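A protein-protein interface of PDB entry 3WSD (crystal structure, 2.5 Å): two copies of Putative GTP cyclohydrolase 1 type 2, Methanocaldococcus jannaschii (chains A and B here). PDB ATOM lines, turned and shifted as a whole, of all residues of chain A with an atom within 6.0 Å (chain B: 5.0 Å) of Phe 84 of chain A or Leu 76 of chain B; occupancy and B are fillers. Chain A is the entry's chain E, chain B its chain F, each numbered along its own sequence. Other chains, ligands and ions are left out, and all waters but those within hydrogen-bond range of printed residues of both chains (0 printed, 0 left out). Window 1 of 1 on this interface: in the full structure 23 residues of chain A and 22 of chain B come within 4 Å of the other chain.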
ATOM      1  N   ILE A  81       7.805  -9.101  28.788  1.00  0.00           N
ATOM      2  CA  ILE A  81       9.217  -8.892  28.473  1.00  0.00           C
ATOM      3  C   ILE A  81       9.505  -7.445  28.050  1.00  0.00           C
ATOM      4  O   ILE A  81       8.584  -6.685  27.715  1.00  0.00           O
ATOM      5  CB  ILE A  81       9.687  -9.826  27.350  1.00  0.00           C
ATOM      6  CG1 ILE A  81       8.944  -9.524  26.047  1.00  0.00           C
ATOM      7  CG2 ILE A  81       9.507 -11.277  27.746  1.00  0.00           C
ATOM      8  CD1 ILE A  81       9.429 -10.358  24.864  1.00  0.00           C
ATOM      9  N   ARG A  82      10.779  -7.061  28.071  1.00  0.00           N
ATOM     10  CA  ARG A  82      11.148  -5.721  27.614  1.00  0.00           C
ATOM     11  C   ARG A  82      12.332  -5.745  26.650  1.00  0.00           C
ATOM     12  O   ARG A  82      12.933  -4.713  26.375  1.00  0.00           O
ATOM     13  CB  ARG A  82      11.450  -4.807  28.808  1.00  0.00           C
ATOM     14  CG  ARG A  82      12.446  -5.353  29.800  1.00  0.00           C
ATOM     15  CD  ARG A  82      12.548  -4.448  31.026  1.00  0.00           C
ATOM     16  NE  ARG A  82      13.736  -4.736  31.817  1.00  0.00           N
ATOM     17  CZ  ARG A  82      14.156  -3.985  32.833  1.00  0.00           C
ATOM     18  NH1 ARG A  82      13.468  -2.909  33.200  1.00  0.00           N
ATOM     19  NH2 ARG A  82      15.259  -4.320  33.491  1.00  0.00           N
ATOM     20  N   ASN A  83      12.659  -6.928  26.139  1.00  0.00           N
ATOM     21  CA  ASN A  83      13.728  -7.080  25.159  1.00  0.00           C
ATOM     22  C   ASN A  83      13.235  -8.034  24.081  1.00  0.00           C
ATOM     23  O   ASN A  83      12.484  -8.966  24.379  1.00  0.00           O
ATOM     24  CB  ASN A  83      14.994  -7.622  25.812  1.00  0.00           C
ATOM     25  CG  ASN A  83      15.594  -6.651  26.819  1.00  0.00           C
ATOM     26  OD1 ASN A  83      15.242  -6.687  27.997  1.00  0.00           O
ATOM     27  ND2 ASN A  83      16.493  -5.787  26.367  1.00  0.00           N
ATOM     28  N   PHE A  84      13.644  -7.807  22.836  1.00  0.00           N
ATOM     29  CA  PHE A  84      13.090  -8.552  21.705  1.00  0.00           C
ATOM     30  C   PHE A  84      14.216  -9.117  20.873  1.00  0.00           C
ATOM     31  O   PHE A  84      14.720  -8.482  19.946  1.00  0.00           O
ATOM     32  CB  PHE A  84      12.174  -7.640  20.893  1.00  0.00           C
ATOM     33  CG  PHE A  84      11.168  -6.942  21.744  1.00  0.00           C
ATOM     34  CD1 PHE A  84       9.998  -7.575  22.117  1.00  0.00           C
ATOM     35  CD2 PHE A  84      11.443  -5.694  22.268  1.00  0.00           C
ATOM     36  CE1 PHE A  84       9.094  -6.947  22.954  1.00  0.00           C
ATOM     37  CE2 PHE A  84      10.541  -5.068  23.100  1.00  0.00           C
ATOM     38  CZ  PHE A  84       9.367  -5.698  23.444  1.00  0.00           C
ATOM     39  N   THR A  85      14.585 -10.342  21.222  1.00  0.00           N
ATOM     40  CA  THR A  85      15.750 -11.018  20.682  1.00  0.00           C
ATOM     41  C   THR A  85      15.416 -12.489  20.509  1.00  0.00           C
ATOM     42  O   THR A  85      14.361 -12.944  20.954  1.00  0.00           O
ATOM     43  CB  THR A  85      16.980 -10.863  21.621  1.00  0.00           C
ATOM     44  OG1 THR A  85      16.678 -11.418  22.907  1.00  0.00           O
ATOM     45  CG2 THR A  85      17.335  -9.403  21.813  1.00  0.00           C
ATOM     46  N   GLY A  86      16.275 -13.218  19.805  1.00  0.00           N
ATOM     47  CA  GLY A  86      16.113 -14.652  19.678  1.00  0.00           C
ATOM     48  C   GLY A  86      14.783 -15.043  19.061  1.00  0.00           C
ATOM     49  O   GLY A  86      14.337 -14.440  18.090  1.00  0.00           O
ATOM     50  N   ILE A  88      11.514 -14.841  20.080  1.00  0.00           N
ATOM     51  CA  ILE A  88      10.418 -13.877  20.053  1.00  0.00           C
ATOM     52  C   ILE A  88      10.670 -12.811  18.975  1.00  0.00           C
ATOM     53  O   ILE A  88       9.723 -12.297  18.369  1.00  0.00           O
ATOM     54  CB  ILE A  88      10.195 -13.201  21.447  1.00  0.00           C
ATOM     55  CG1 ILE A  88       8.823 -12.517  21.494  1.00  0.00           C
ATOM     56  CG2 ILE A  88      11.334 -12.237  21.811  1.00  0.00           C
ATOM     57  CD1 ILE A  88       7.667 -13.467  21.325  1.00  0.00           C
ATOM     58  N   TYR A  89      11.944 -12.506  18.713  1.00  0.00           N
ATOM     59  CA  TYR A  89      12.284 -11.591  17.636  1.00  0.00           C
ATOM     60  C   TYR A  89      11.875 -12.202  16.292  1.00  0.00           C
ATOM     61  O   TYR A  89      11.303 -11.514  15.441  1.00  0.00           O
ATOM     62  CB  TYR A  89      13.782 -11.241  17.642  1.00  0.00           C
ATOM     63  CG  TYR A  89      14.182 -10.320  16.499  1.00  0.00           C
ATOM     64  CD1 TYR A  89      14.561 -10.835  15.257  1.00  0.00           C
ATOM     65  CD2 TYR A  89      14.122  -8.940  16.642  1.00  0.00           C
ATOM     66  CE1 TYR A  89      14.902  -9.997  14.201  1.00  0.00           C
ATOM     67  CE2 TYR A  89      14.456  -8.097  15.589  1.00  0.00           C
ATOM     68  CZ  TYR A  89      14.847  -8.631  14.374  1.00  0.00           C
ATOM     69  OH  TYR A  89      15.176  -7.793  13.332  1.00  0.00           O
ATOM     70  N   LEU A  92       7.786 -12.187  16.007  1.00  0.00           N
ATOM     71  CA  LEU A  92       7.201 -10.856  15.847  1.00  0.00           C
ATOM     72  C   LEU A  92       7.543 -10.281  14.487  1.00  0.00           C
ATOM     73  O   LEU A  92       6.727  -9.592  13.875  1.00  0.00           O
ATOM     74  CB  LEU A  92       7.681  -9.908  16.955  1.00  0.00           C
ATOM     75  CG  LEU A  92       7.218 -10.221  18.384  1.00  0.00           C
ATOM     76  CD1 LEU A  92       7.821  -9.253  19.375  1.00  0.00           C
ATOM     77  CD2 LEU A  92       5.709 -10.159  18.470  1.00  0.00           C
ATOM     78  N   GLN B  36      18.239  -4.119  22.685  1.00  0.00           N
ATOM     79  CA  GLN B  36      16.805  -3.883  22.849  1.00  0.00           C
ATOM     80  C   GLN B  36      16.015  -4.703  21.844  1.00  0.00           C
ATOM     81  O   GLN B  36      15.102  -5.453  22.212  1.00  0.00           O
ATOM     82  CB  GLN B  36      16.474  -2.394  22.674  1.00  0.00           C
ATOM     83  CG  GLN B  36      17.327  -1.473  23.531  1.00  0.00           C
ATOM     84  CD  GLN B  36      17.019  -1.599  25.017  1.00  0.00           C
ATOM     85  OE1 GLN B  36      15.902  -1.327  25.461  1.00  0.00           O
ATOM     86  NE2 GLN B  36      18.008  -2.037  25.787  1.00  0.00           N
ATOM     87  N   VAL B  37      16.370  -4.541  20.566  1.00  0.00           N
ATOM     88  CA  VAL B  37      15.719  -5.252  19.466  1.00  0.00           C
ATOM     89  C   VAL B  37      16.768  -5.745  18.494  1.00  0.00           C
ATOM     90  O   VAL B  37      17.531  -4.955  17.958  1.00  0.00           O
ATOM     91  CB  VAL B  37      14.727  -4.348  18.690  1.00  0.00           C
ATOM     92  CG1 VAL B  37      14.121  -5.106  17.517  1.00  0.00           C
ATOM     93  CG2 VAL B  37      13.629  -3.820  19.595  1.00  0.00           C
ATOM     94  N   GLY B  38      16.839  -7.046  18.269  1.00  0.00           N
ATOM     95  CA  GLY B  38      17.805  -7.541  17.309  1.00  0.00           C
ATOM     96  C   GLY B  38      18.101  -9.016  17.418  1.00  0.00           C
ATOM     97  O   GLY B  38      17.963  -9.611  18.481  1.00  0.00           O
ATOM     98  N   PRO B  54      14.691   6.312  22.000  1.00  0.00           N
ATOM     99  CA  PRO B  54      14.175   5.468  20.917  1.00  0.00           C
ATOM    100  C   PRO B  54      12.719   5.826  20.602  1.00  0.00           C
ATOM    101  O   PRO B  54      11.859   4.946  20.671  1.00  0.00           O
ATOM    102  CB  PRO B  54      14.270   4.053  21.495  1.00  0.00           C
ATOM    103  CG  PRO B  54      14.109   4.263  22.996  1.00  0.00           C
ATOM    104  CD  PRO B  54      14.618   5.653  23.320  1.00  0.00           C
ATOM    105  N   ILE B  59      12.914   6.517  15.232  1.00  0.00           N
ATOM    106  CA  ILE B  59      12.953   5.248  14.520  1.00  0.00           C
ATOM    107  C   ILE B  59      12.533   5.435  13.052  1.00  0.00           C
ATOM    108  O   ILE B  59      13.138   4.841  12.162  1.00  0.00           O
ATOM    109  CB  ILE B  59      12.060   4.194  15.233  1.00  0.00           C
ATOM    110  CG1 ILE B  59      12.721   3.763  16.547  1.00  0.00           C
ATOM    111  CG2 ILE B  59      11.816   2.978  14.362  1.00  0.00           C
ATOM    112  CD1 ILE B  59      11.844   2.912  17.439  1.00  0.00           C
ATOM    113  N   HIS B  74      18.343   6.004  26.271  1.00  0.00           N
ATOM    114  CA  HIS B  74      17.238   5.410  27.013  1.00  0.00           C
ATOM    115  C   HIS B  74      16.796   4.099  26.390  1.00  0.00           C
ATOM    116  O   HIS B  74      16.739   3.980  25.171  1.00  0.00           O
ATOM    117  CB  HIS B  74      16.068   6.386  27.105  1.00  0.00           C
ATOM    118  CG  HIS B  74      16.415   7.651  27.822  1.00  0.00           C
ATOM    119  ND1 HIS B  74      16.471   8.874  27.189  1.00  0.00           N
ATOM    120  CD2 HIS B  74      16.793   7.872  29.102  1.00  0.00           C
ATOM    121  CE1 HIS B  74      16.833   9.799  28.057  1.00  0.00           C
ATOM    122  NE2 HIS B  74      17.044   9.217  29.223  1.00  0.00           N
ATOM    123  N   PRO B  75      16.491   3.106  27.236  1.00  0.00           N
ATOM    124  CA  PRO B  75      15.972   1.820  26.751  1.00  0.00           C
ATOM    125  C   PRO B  75      14.623   2.003  26.060  1.00  0.00           C
ATOM    126  O   PRO B  75      13.948   3.012  26.300  1.00  0.00           O
ATOM    127  CB  PRO B  75      15.818   0.987  28.032  1.00  0.00           C
ATOM    128  CG  PRO B  75      16.666   1.681  29.056  1.00  0.00           C
ATOM    129  CD  PRO B  75      16.662   3.130  28.699  1.00  0.00           C
ATOM    130  N   LEU B  76      14.251   1.042  25.217  1.00  0.00           N
ATOM    131  CA  LEU B  76      12.969   1.054  24.524  1.00  0.00           C
ATOM    132  C   LEU B  76      11.803   0.971  25.499  1.00  0.00           C
ATOM    133  O   LEU B  76      10.814   1.670  25.338  1.00  0.00           O
ATOM    134  CB  LEU B  76      12.883  -0.110  23.527  1.00  0.00           C
ATOM    135  CG  LEU B  76      11.634  -0.240  22.644  1.00  0.00           C
ATOM    136  CD1 LEU B  76      11.447   0.960  21.716  1.00  0.00           C
ATOM    137  CD2 LEU B  76      11.664  -1.529  21.836  1.00  0.00           C
ATOM    138  N   LEU B  77      11.920   0.099  26.497  1.00  0.00           N
ATOM    139  CA  LEU B  77      10.858  -0.111  27.478  1.00  0.00           C
ATOM    140  C   LEU B  77      11.423  -0.204  28.885  1.00  0.00           C
ATOM    141  O   LEU B  77      12.458  -0.825  29.105  1.00  0.00           O
ATOM    142  CB  LEU B  77      10.067  -1.392  27.175  1.00  0.00           C
ATOM    143  CG  LEU B  77       9.238  -1.542  25.897  1.00  0.00           C
ATOM    144  CD1 LEU B  77       8.777  -2.982  25.750  1.00  0.00           C
ATOM    145  CD2 LEU B  77       8.030  -0.611  25.919  1.00  0.00           C
ATOM    146  N   LYS B  78      10.758   0.427  29.841  1.00  0.00           N
ATOM    147  CA  LYS B  78      11.099   0.205  31.241  1.00  0.00           C
ATOM    148  C   LYS B  78      10.130  -0.795  31.846  1.00  0.00           C
ATOM    149  O   LYS B  78      10.540  -1.708  32.559  1.00  0.00           O
ATOM    150  CB  LYS B  78      11.138   1.526  32.020  1.00  0.00           C
ATOM    151  CG  LYS B  78      12.500   2.216  31.869  1.00  0.00           C
ATOM    152  CD  LYS B  78      12.474   3.732  32.002  1.00  0.00           C
ATOM    153  CE  LYS B  78      13.821   4.311  31.545  1.00  0.00           C
ATOM    154  NZ  LYS B  78      13.731   5.563  30.737  1.00  0.00           N
ATOM    155  N   ILE B  81       6.080  -5.868  28.766  1.00  0.00           N
ATOM    156  CA  ILE B  81       4.771  -6.063  28.138  1.00  0.00           C
ATOM    157  C   ILE B  81       4.611  -7.493  27.618  1.00  0.00           C
ATOM    158  O   ILE B  81       5.590  -8.231  27.467  1.00  0.00           O
ATOM    159  CB  ILE B  81       4.540  -5.081  26.946  1.00  0.00           C
ATOM    160  CG1 ILE B  81       5.543  -5.334  25.811  1.00  0.00           C
ATOM    161  CG2 ILE B  81       4.609  -3.635  27.410  1.00  0.00           C
ATOM    162  CD1 ILE B  81       5.323  -4.462  24.575  1.00  0.00           C
ATOM    163  N   PHE B  84       1.238  -6.667  21.898  1.00  0.00           N
ATOM    164  CA  PHE B  84       1.904  -5.791  20.932  1.00  0.00           C
ATOM    165  C   PHE B  84       0.955  -5.056  20.021  1.00  0.00           C
ATOM    166  O   PHE B  84       0.529  -5.576  18.997  1.00  0.00           O
ATOM    167  CB  PHE B  84       2.891  -6.608  20.115  1.00  0.00           C
ATOM    168  CG  PHE B  84       3.849  -7.353  20.962  1.00  0.00           C
ATOM    169  CD1 PHE B  84       4.989  -6.730  21.437  1.00  0.00           C
ATOM    170  CD2 PHE B  84       3.554  -8.633  21.385  1.00  0.00           C
ATOM    171  CE1 PHE B  84       5.856  -7.398  22.255  1.00  0.00           C
ATOM    172  CE2 PHE B  84       4.408  -9.307  22.212  1.00  0.00           C
ATOM    173  CZ  PHE B  84       5.565  -8.692  22.649  1.00  0.00           C
ATOM    174  N   ILE B  88       4.019   0.796  20.322  1.00  0.00           N
ATOM    175  CA  ILE B  88       5.088  -0.190  20.389  1.00  0.00           C
ATOM    176  C   ILE B  88       5.034  -1.126  19.173  1.00  0.00           C
ATOM    177  O   ILE B  88       6.071  -1.601  18.706  1.00  0.00           O
ATOM    178  CB  ILE B  88       5.040  -1.002  21.712  1.00  0.00           C
ATOM    179  CG1 ILE B  88       6.337  -1.779  21.905  1.00  0.00           C
ATOM    180  CG2 ILE B  88       3.833  -1.938  21.761  1.00  0.00           C
ATOM    181  CD1 ILE B  88       7.556  -0.892  22.008  1.00  0.00           C
ATOM    182  N   LYS B  91       6.764   0.799  16.328  1.00  0.00           N
ATOM    183  CA  LYS B  91       8.205   0.857  16.523  1.00  0.00           C
ATOM    184  C   LYS B  91       8.880  -0.441  16.114  1.00  0.00           C
ATOM    185  O   LYS B  91       9.877  -0.427  15.387  1.00  0.00           O
ATOM    186  CB  LYS B  91       8.537   1.168  17.967  1.00  0.00           C
ATOM    187  CG  LYS B  91       8.129   2.546  18.415  1.00  0.00           C
ATOM    188  CD  LYS B  91       8.602   2.715  19.837  1.00  0.00           C
ATOM    189  CE  LYS B  91       8.436   4.119  20.320  1.00  0.00           C
ATOM    190  NZ  LYS B  91       9.150   4.319  21.607  1.00  0.00           N
ATOM    191  N   LEU B  92       8.351  -1.562  16.596  1.00  0.00           N
ATOM    192  CA  LEU B  92       8.955  -2.858  16.300  1.00  0.00           C
ATOM    193  C   LEU B  92       8.845  -3.211  14.824  1.00  0.00           C
ATOM    194  O   LEU B  92       9.787  -3.754  14.235  1.00  0.00           O
ATOM    195  CB  LEU B  92       8.309  -3.950  17.138  1.00  0.00           C
ATOM    196  CG  LEU B  92       8.606  -3.739  18.614  1.00  0.00           C
ATOM    197  CD1 LEU B  92       7.926  -4.801  19.447  1.00  0.00           C
ATOM    198  CD2 LEU B  92      10.120  -3.705  18.855  1.00  0.00           C
ATOM    199  N   MET B  96      12.024  -4.125  12.686  1.00  0.00           N
ATOM    200  CA  MET B  96      12.186  -5.513  12.255  1.00  0.00           C
ATOM    201  C   MET B  96      12.185  -5.736  10.752  1.00  0.00           C
ATOM    202  O   MET B  96      12.996  -6.507  10.250  1.00  0.00           O
ATOM    203  CB  MET B  96      11.101  -6.376  12.888  1.00  0.00           C
ATOM    204  CG  MET B  96      11.373  -6.639  14.361  1.00  0.00           C
ATOM    205  SD  MET B  96       9.998  -7.380  15.225  1.00  0.00           S
ATOM    206  CE  MET B  96      10.709  -7.601  16.860  1.00  0.00           C
ATOM    207  N   LEU B 102      18.588  -2.228  17.536  1.00  0.00           N
ATOM    208  CA  LEU B 102      18.460  -1.194  18.557  1.00  0.00           C
ATOM    209  C   LEU B 102      19.229  -1.617  19.810  1.00  0.00           C
ATOM    210  O   LEU B 102      18.964  -2.665  20.398  1.00  0.00           O
ATOM    211  CB  LEU B 102      16.992  -0.926  18.893  1.00  0.00           C
ATOM    212  CG  LEU B 102      16.759   0.119  19.986  1.00  0.00           C
ATOM    213  CD1 LEU B 102      17.324   1.455  19.545  1.00  0.00           C
ATOM    214  CD2 LEU B 102      15.294   0.239  20.365  1.00  0.00           C
ATOM    215  N   SER B 104      21.181  -0.164  23.597  1.00  0.00           N
ATOM    216  CA  SER B 104      21.210   0.923  24.579  1.00  0.00           C
ATOM    217  C   SER B 104      22.300   0.829  25.634  1.00  0.00           C
ATOM    218  O   SER B 104      22.609  -0.245  26.158  1.00  0.00           O
ATOM    219  CB  SER B 104      19.868   1.037  25.310  1.00  0.00           C
ATOM    220  OG  SER B 104      18.823   1.350  24.410  1.00  0.00           O
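The backbone carbonyl oxygen (O) of Phe 84 of chain A sits at hydrogen-bond distance from the backbone NH (N) of Gly 38 of chain B, at 3.1 Å. The backbone carbonyl oxygen of Lys 78 of chain B sits at hydrogen-bond distance from the guanidinium group of Arg 82 of chain A (3.2 Å). The backbone NH (N) of Phe 84 of chain A is in hydrogen-bond range of the backbone carbonyl oxygen (O) of Gln 36 of chain B (2.8 Å). The backbone NH (N) of Ile 81 of chain A lies within hydrogen-bond range of the backbone carbonyl oxygen (O) of Ile 81 of chain B (2.7 Å).
The backbone NH (N) of Gln 36 of chain B lies within hydrogen-bond range of the backbone carbonyl oxygen (O) of Leu 102 of chain B, at 2.8 Å. The backbone carbonyl oxygen of Val 37 of chain B sits at hydrogen-bond distance from the backbone NH of Leu 102 of chain B, 3.0 Å away. The backbone NH of Leu 76 of chain B lies within hydrogen-bond range of the side-chain amide oxygen of Gln 36 of chain B, at 2.9 Å.
Among the printed residues, pairs that only touch across the chains: Asn 83 of chain A with Gln 36 of chain B, Phe 84 of chain A with Val 37 of chain B, Phe 84 of chain A with Leu 76 of chain B, Phe 84 of chain A with Leu 77 of chain B, Phe 84 of chain A with Phe 84 of chain B, Thr 85 of chain A with Gly 38 of chain B, Tyr 89 of chain A with Val 37 of chain B, Tyr 89 of chain A with Gly 38 of chain B, Tyr 89 of chain A with Met 96 of chain B, Leu 92 of chain A with Phe 84 of chain B and Leu 92 of chain A with Met 96 of chain B.
Phe 84 of chain A touches six residues of chain B. Of chain A, only Phe 84 comes within 4 Å of Leu 76 of chain B. Of the printed residues of chain A, Lys 78 of chain B touches Arg 82. Of the printed residues of chain A, Phe 84 of chain B touches Phe 84 and Leu 92. Pro 75 of chain B touches none of the printed residues of chain A. The nearest residue of chain B that does not touch Phe 84 of chain A is Leu 92 of chain B (4.2 Å). The nearest residue of chain A that does not touch Leu 76 of chain B is Arg 82 of chain A (5.4 Å).
Along chain A the printed residues that touch a printed residue of chain B span positions 81 to 92. Among the printed residues, no Asp or Glu carboxylate lies within 4 Å of a Lys or Arg side-chain nitrogen of the other chain.
Ile 81 of chain B touches its own counterpart, Ile 81 of chain A. Phe 84 of chain A touches its own counterpart, Phe 84 of chain B. Leu 92 of chain A touches Phe 84 of chain B, but with the chains exchanged Phe 84 of chain A does not touch Leu 92 of chain B (4.2 Å). Positions printed for both chains: 81, 84, 88 and 92.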
